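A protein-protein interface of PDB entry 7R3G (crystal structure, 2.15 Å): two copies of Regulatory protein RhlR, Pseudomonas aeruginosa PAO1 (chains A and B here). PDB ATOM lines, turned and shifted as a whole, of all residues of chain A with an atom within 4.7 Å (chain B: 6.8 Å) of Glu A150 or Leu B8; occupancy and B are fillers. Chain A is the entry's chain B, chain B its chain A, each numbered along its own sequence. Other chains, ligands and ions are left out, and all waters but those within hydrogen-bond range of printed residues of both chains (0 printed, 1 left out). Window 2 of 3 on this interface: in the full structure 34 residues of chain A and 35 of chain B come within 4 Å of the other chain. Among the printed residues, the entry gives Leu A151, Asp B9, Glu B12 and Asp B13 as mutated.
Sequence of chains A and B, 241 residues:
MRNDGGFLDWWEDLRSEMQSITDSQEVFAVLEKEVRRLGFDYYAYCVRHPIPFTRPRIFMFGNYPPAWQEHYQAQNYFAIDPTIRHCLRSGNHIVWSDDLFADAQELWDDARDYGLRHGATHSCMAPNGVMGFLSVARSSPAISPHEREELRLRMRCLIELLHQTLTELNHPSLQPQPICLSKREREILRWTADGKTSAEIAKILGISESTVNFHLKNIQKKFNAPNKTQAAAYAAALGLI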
ATOM      1  N   PHE A   7      15.166  22.645 -15.277  1.00  0.00           N
ATOM      2  CA  PHE A   7      14.128  21.995 -16.073  1.00  0.00           C
ATOM      3  C   PHE A   7      14.519  20.565 -16.428  1.00  0.00           C
ATOM      4  O   PHE A   7      13.661  19.677 -16.497  1.00  0.00           O
ATOM      5  CB  PHE A   7      13.859  22.798 -17.347  1.00  0.00           C
ATOM      6  CG  PHE A   7      12.839  22.165 -18.262  1.00  0.00           C
ATOM      7  CD1 PHE A   7      13.207  21.171 -19.157  1.00  0.00           C
ATOM      8  CD2 PHE A   7      11.516  22.566 -18.225  1.00  0.00           C
ATOM      9  CE1 PHE A   7      12.273  20.587 -19.992  1.00  0.00           C
ATOM     10  CE2 PHE A   7      10.577  21.987 -19.060  1.00  0.00           C
ATOM     11  CZ  PHE A   7      10.957  20.997 -19.945  1.00  0.00           C
ATOM     12  N   GLU A 147       4.603  33.221 -17.549  1.00  0.00           N
ATOM     13  CA  GLU A 147       4.641  31.783 -17.320  1.00  0.00           C
ATOM     14  C   GLU A 147       4.149  30.978 -18.518  1.00  0.00           C
ATOM     15  O   GLU A 147       4.230  29.746 -18.493  1.00  0.00           O
ATOM     16  CB  GLU A 147       3.804  31.429 -16.075  1.00  0.00           C
ATOM     17  CG  GLU A 147       2.282  31.476 -16.276  1.00  0.00           C
ATOM     18  CD  GLU A 147       1.492  30.956 -15.074  1.00  0.00           C
ATOM     19  OE1 GLU A 147       1.611  29.753 -14.754  1.00  0.00           O
ATOM     20  OE2 GLU A 147       0.735  31.746 -14.462  1.00  0.00           O
ATOM     21  N   ARG A 148       3.689  31.643 -19.579  1.00  0.00           N
ATOM     22  CA  ARG A 148       2.989  30.942 -20.650  1.00  0.00           C
ATOM     23  C   ARG A 148       3.904  29.970 -21.380  1.00  0.00           C
ATOM     24  O   ARG A 148       3.571  28.790 -21.542  1.00  0.00           O
ATOM     25  CB  ARG A 148       2.406  31.953 -21.635  1.00  0.00           C
ATOM     26  CG  ARG A 148       1.010  32.409 -21.295  1.00  0.00           C
ATOM     27  CD  ARG A 148       0.617  33.617 -22.122  1.00  0.00           C
ATOM     28  NE  ARG A 148      -0.790  33.940 -21.937  1.00  0.00           N
ATOM     29  CZ  ARG A 148      -1.760  33.581 -22.766  1.00  0.00           C
ATOM     30  NH1 ARG A 148      -1.508  32.922 -23.885  1.00  0.00           N
ATOM     31  NH2 ARG A 148      -3.016  33.889 -22.461  1.00  0.00           N
ATOM     32  N   GLU A 149       5.059  30.447 -21.843  1.00  0.00           N
ATOM     33  CA  GLU A 149       5.918  29.600 -22.663  1.00  0.00           C
ATOM     34  C   GLU A 149       6.443  28.409 -21.872  1.00  0.00           C
ATOM     35  O   GLU A 149       6.562  27.303 -22.413  1.00  0.00           O
ATOM     36  CB  GLU A 149       7.066  30.425 -23.243  1.00  0.00           C
ATOM     37  CG  GLU A 149       6.758  31.009 -24.619  1.00  0.00           C
ATOM     38  CD  GLU A 149       6.488  29.940 -25.668  1.00  0.00           C
ATOM     39  OE1 GLU A 149       6.948  28.792 -25.482  1.00  0.00           O
ATOM     40  OE2 GLU A 149       5.816  30.247 -26.675  1.00  0.00           O
ATOM     41  N   GLU A 150       6.753  28.604 -20.588  1.00  0.00           N
ATOM     42  CA  GLU A 150       7.191  27.474 -19.772  1.00  0.00           C
ATOM     43  C   GLU A 150       6.047  26.494 -19.536  1.00  0.00           C
ATOM     44  O   GLU A 150       6.262  25.279 -19.478  1.00  0.00           O
ATOM     45  CB  GLU A 150       7.755  27.956 -18.437  1.00  0.00           C
ATOM     46  CG  GLU A 150       8.225  26.814 -17.537  1.00  0.00           C
ATOM     47  CD  GLU A 150       9.071  27.285 -16.366  1.00  0.00           C
ATOM     48  OE1 GLU A 150       9.253  28.510 -16.215  1.00  0.00           O
ATOM     49  OE2 GLU A 150       9.552  26.423 -15.599  1.00  0.00           O
ATOM     50  N   LEU A 151       4.823  27.008 -19.387  1.00  0.00           N
ATOM     51  CA  LEU A 151       3.674  26.126 -19.226  1.00  0.00           C
ATOM     52  C   LEU A 151       3.462  25.275 -20.470  1.00  0.00           C
ATOM     53  O   LEU A 151       3.199  24.072 -20.372  1.00  0.00           O
ATOM     54  CB  LEU A 151       2.424  26.951 -18.924  1.00  0.00           C
ATOM     55  CG  LEU A 151       1.125  26.167 -18.772  1.00  0.00           C
ATOM     56  CD1 LEU A 151       1.187  25.284 -17.537  1.00  0.00           C
ATOM     57  CD2 LEU A 151      -0.059  27.119 -18.706  1.00  0.00           C
ATOM     58  N   ARG A 152       3.563  25.887 -21.650  1.00  0.00           N
ATOM     59  CA  ARG A 152       3.476  25.123 -22.890  1.00  0.00           C
ATOM     60  C   ARG A 152       4.473  23.973 -22.886  1.00  0.00           C
ATOM     61  O   ARG A 152       4.110  22.812 -23.111  1.00  0.00           O
ATOM     62  CB  ARG A 152       3.725  26.053 -24.079  1.00  0.00           C
ATOM     63  CG  ARG A 152       3.438  25.433 -25.433  1.00  0.00           C
ATOM     64  CD  ARG A 152       2.919  26.475 -26.416  1.00  0.00           C
ATOM     65  NE  ARG A 152       3.925  26.881 -27.391  1.00  0.00           N
ATOM     66  CZ  ARG A 152       4.439  26.082 -28.315  1.00  0.00           C
ATOM     67  NH1 ARG A 152       4.093  24.807 -28.394  1.00  0.00           N
ATOM     68  NH2 ARG A 152       5.320  26.573 -29.182  1.00  0.00           N
ATOM     69  N   LEU A 153       5.741  24.284 -22.607  1.00  0.00           N
ATOM     70  CA  LEU A 153       6.797  23.279 -22.665  1.00  0.00           C
ATOM     71  C   LEU A 153       6.568  22.172 -21.650  1.00  0.00           C
ATOM     72  O   LEU A 153       6.747  20.988 -21.959  1.00  0.00           O
ATOM     73  CB  LEU A 153       8.150  23.946 -22.412  1.00  0.00           C
ATOM     74  CG  LEU A 153       9.029  24.162 -23.639  1.00  0.00           C
ATOM     75  CD1 LEU A 153       9.363  22.841 -24.286  1.00  0.00           C
ATOM     76  CD2 LEU A 153       8.317  25.084 -24.608  1.00  0.00           C
ATOM     77  N   ARG A 154       6.191  22.539 -20.427  1.00  0.00           N
ATOM     78  CA  ARG A 154       5.926  21.542 -19.401  1.00  0.00           C
ATOM     79  C   ARG A 154       4.717  20.691 -19.758  1.00  0.00           C
ATOM     80  O   ARG A 154       4.719  19.474 -19.540  1.00  0.00           O
ATOM     81  CB  ARG A 154       5.717  22.236 -18.058  1.00  0.00           C
ATOM     82  CG  ARG A 154       6.950  22.956 -17.543  1.00  0.00           C
ATOM     83  CD  ARG A 154       7.765  22.053 -16.636  1.00  0.00           C
ATOM     84  NE  ARG A 154       7.242  22.065 -15.276  1.00  0.00           N
ATOM     85  CZ  ARG A 154       7.504  23.009 -14.384  1.00  0.00           C
ATOM     86  NH1 ARG A 154       8.313  24.018 -14.665  1.00  0.00           N
ATOM     87  NH2 ARG A 154       6.939  22.941 -13.182  1.00  0.00           N
ATOM     88  N   GLY B   6      20.914  27.569 -18.766  1.00  0.00           N
ATOM     89  CA  GLY B   6      20.459  26.195 -18.858  1.00  0.00           C
ATOM     90  C   GLY B   6      19.568  25.939 -20.057  1.00  0.00           C
ATOM     91  O   GLY B   6      19.661  26.635 -21.067  1.00  0.00           O
ATOM     92  N   PHE B   7      18.691  24.940 -19.936  1.00  0.00           N
ATOM     93  CA  PHE B   7      17.843  24.554 -21.061  1.00  0.00           C
ATOM     94  C   PHE B   7      16.838  25.649 -21.399  1.00  0.00           C
ATOM     95  O   PHE B   7      16.668  26.008 -22.570  1.00  0.00           O
ATOM     96  CB  PHE B   7      17.118  23.244 -20.747  1.00  0.00           C
ATOM     97  CG  PHE B   7      16.233  22.762 -21.861  1.00  0.00           C
ATOM     98  CD1 PHE B   7      16.742  21.968 -22.873  1.00  0.00           C
ATOM     99  CD2 PHE B   7      14.894  23.110 -21.900  1.00  0.00           C
ATOM    100  CE1 PHE B   7      15.934  21.527 -23.903  1.00  0.00           C
ATOM    101  CE2 PHE B   7      14.079  22.672 -22.927  1.00  0.00           C
ATOM    102  CZ  PHE B   7      14.601  21.879 -23.930  1.00  0.00           C
ATOM    103  N   LEU B   8      16.152  26.187 -20.386  1.00  0.00           N
ATOM    104  CA  LEU B   8      15.139  27.209 -20.642  1.00  0.00           C
ATOM    105  C   LEU B   8      15.765  28.477 -21.209  1.00  0.00           C
ATOM    106  O   LEU B   8      15.149  29.166 -22.031  1.00  0.00           O
ATOM    107  CB  LEU B   8      14.379  27.530 -19.357  1.00  0.00           C
ATOM    108  CG  LEU B   8      13.193  26.652 -18.958  1.00  0.00           C
ATOM    109  CD1 LEU B   8      12.290  27.437 -18.000  1.00  0.00           C
ATOM    110  CD2 LEU B   8      12.385  26.159 -20.141  1.00  0.00           C
ATOM    111  N   ASP B   9      16.976  28.819 -20.763  1.00  0.00           N
ATOM    112  CA  ASP B   9      17.704  29.920 -21.381  1.00  0.00           C
ATOM    113  C   ASP B   9      17.914  29.652 -22.868  1.00  0.00           C
ATOM    114  O   ASP B   9      17.597  30.495 -23.716  1.00  0.00           O
ATOM    115  CB  ASP B   9      19.043  30.126 -20.669  1.00  0.00           C
ATOM    116  CG  ASP B   9      18.881  30.653 -19.249  1.00  0.00           C
ATOM    117  OD1 ASP B   9      17.816  31.229 -18.939  1.00  0.00           O
ATOM    118  OD2 ASP B   9      19.825  30.494 -18.445  1.00  0.00           O
ATOM    119  N   TRP B  10      18.433  28.468 -23.200  1.00  0.00           N
ATOM    120  CA  TRP B  10      18.643  28.110 -24.599  1.00  0.00           C
ATOM    121  C   TRP B  10      17.349  28.231 -25.394  1.00  0.00           C
ATOM    122  O   TRP B  10      17.319  28.830 -26.476  1.00  0.00           O
ATOM    123  CB  TRP B  10      19.195  26.686 -24.691  1.00  0.00           C
ATOM    124  CG  TRP B  10      19.202  26.122 -26.082  1.00  0.00           C
ATOM    125  CD1 TRP B  10      20.161  26.309 -27.033  1.00  0.00           C
ATOM    126  CD2 TRP B  10      18.206  25.281 -26.680  1.00  0.00           C
ATOM    127  NE1 TRP B  10      19.826  25.639 -28.182  1.00  0.00           N
ATOM    128  CE2 TRP B  10      18.630  24.999 -27.993  1.00  0.00           C
ATOM    129  CE3 TRP B  10      16.999  24.738 -26.232  1.00  0.00           C
ATOM    130  CZ2 TRP B  10      17.891  24.201 -28.862  1.00  0.00           C
ATOM    131  CZ3 TRP B  10      16.266  23.946 -27.097  1.00  0.00           C
ATOM    132  CH2 TRP B  10      16.715  23.685 -28.396  1.00  0.00           C
ATOM    133  N   TRP B  11      16.265  27.671 -24.861  1.00  0.00           N
ATOM    134  CA  TRP B  11      14.997  27.659 -25.582  1.00  0.00           C
ATOM    135  C   TRP B  11      14.489  29.075 -25.822  1.00  0.00           C
ATOM    136  O   TRP B  11      14.073  29.416 -26.935  1.00  0.00           O
ATOM    137  CB  TRP B  11      13.979  26.833 -24.799  1.00  0.00           C
ATOM    138  CG  TRP B  11      12.605  26.847 -25.371  1.00  0.00           C
ATOM    139  CD1 TRP B  11      11.454  27.173 -24.718  1.00  0.00           C
ATOM    140  CD2 TRP B  11      12.226  26.510 -26.710  1.00  0.00           C
ATOM    141  NE1 TRP B  11      10.382  27.069 -25.568  1.00  0.00           N
ATOM    142  CE2 TRP B  11      10.828  26.659 -26.797  1.00  0.00           C
ATOM    143  CE3 TRP B  11      12.933  26.098 -27.846  1.00  0.00           C
ATOM    144  CZ2 TRP B  11      10.122  26.413 -27.974  1.00  0.00           C
ATOM    145  CZ3 TRP B  11      12.230  25.856 -29.015  1.00  0.00           C
ATOM    146  CH2 TRP B  11      10.839  26.011 -29.068  1.00  0.00           C
ATOM    147  N   GLU B  12      14.522  29.921 -24.790  1.00  0.00           N
ATOM    148  CA  GLU B  12      13.995  31.274 -24.938  1.00  0.00           C
ATOM    149  C   GLU B  12      14.826  32.087 -25.923  1.00  0.00           C
ATOM    150  O   GLU B  12      14.281  32.898 -26.682  1.00  0.00           O
ATOM    151  CB  GLU B  12      13.943  31.973 -23.579  1.00  0.00           C
ATOM    152  N   ASP B  13      16.146  31.888 -25.927  1.00  0.00           N
ATOM    153  CA  ASP B  13      16.996  32.617 -26.863  1.00  0.00           C
ATOM    154  C   ASP B  13      16.727  32.187 -28.300  1.00  0.00           C
ATOM    155  O   ASP B  13      16.772  33.012 -29.220  1.00  0.00           O
ATOM    156  CB  ASP B  13      18.468  32.407 -26.510  1.00  0.00           C
ATOM    157  CG  ASP B  13      18.903  33.226 -25.309  1.00  0.00           C
ATOM    158  OD1 ASP B  13      18.425  34.370 -25.162  1.00  0.00           O
ATOM    159  OD2 ASP B  13      19.726  32.726 -24.513  1.00  0.00           O
ATOM    160  N   ARG B  15      13.794  30.830 -29.461  1.00  0.00           N
ATOM    161  CA  ARG B  15      12.496  31.408 -29.789  1.00  0.00           C
ATOM    162  C   ARG B  15      12.657  32.853 -30.244  1.00  0.00           C
ATOM    163  O   ARG B  15      12.132  33.256 -31.287  1.00  0.00           O
ATOM    164  CB  ARG B  15      11.563  31.326 -28.580  1.00  0.00           C
ATOM    165  CG  ARG B  15      10.999  29.940 -28.308  1.00  0.00           C
ATOM    166  CD  ARG B  15       9.742  30.012 -27.448  1.00  0.00           C
ATOM    167  NE  ARG B  15      10.031  30.384 -26.066  1.00  0.00           N
ATOM    168  CZ  ARG B  15      10.011  31.626 -25.599  1.00  0.00           C
ATOM    169  NH1 ARG B  15       9.722  32.655 -26.380  1.00  0.00           N
ATOM    170  NH2 ARG B  15      10.280  31.840 -24.313  1.00  0.00           N
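The guanidinium group of Arg B15 is in salt-bridge range of the side-chain carboxylate of Glu A149 (3.5 Å).
Phe A7 touches its own counterpart, Phe B7. Position printed for both chains: 7. Of the 5 pairs that touch across the chains among the printed residues, 1 has its exchanged pair printed and touching as well.
Printed residues of chain B within 4 Å of Glu A150: Leu B8. Of chain A, only Glu A150 (3.6 Å) comes within 4 Å of Leu B8. Of the printed residues of chain A, Arg B15 touches Glu A149. Of the printed residues of chain B, Phe A7 touches Phe B7. Printed residues of chain A within 4 Å of Trp B11: Glu A149 (3.8 Å) and Leu A153 (3.0 Å). Of the printed residues of chain B, Glu A149 touches Trp B11 (3.8 Å) and Arg B15 (3.5 Å). The nearest residue of chain A that does not touch Leu B8 is Phe A7 (4.2 Å).
OE2 of Glu A150 is in salt-bridge range of NH1 of Arg A154, at 2.9 Å. The side-chain carboxylate (OE2) of Glu A149 lies within salt-bridge range of the guanidinium group (NE) of Arg A152, 3.9 Å away.
Among the printed residues, merely in contact across the chains: Phe A7 with Phe B7, Glu A149 with Trp B11, Glu A150 with Leu B8 and Leu A153 with Trp B11.
Hydrophobic or aromatic side chains of chain B within 4 Å of the printed part of chain A: Phe B7, Leu B8 and Trp B11. Hydrophobic or aromatic side chains of chain A within 4 Å of the printed part of chain B: Phe A7 and Leu A153. Among the printed residues, Asp or Glu carboxylates within 4 Å of a Lys or Arg side-chain nitrogen of the other chain: Glu A149 with Arg B15 (3.5 Å).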
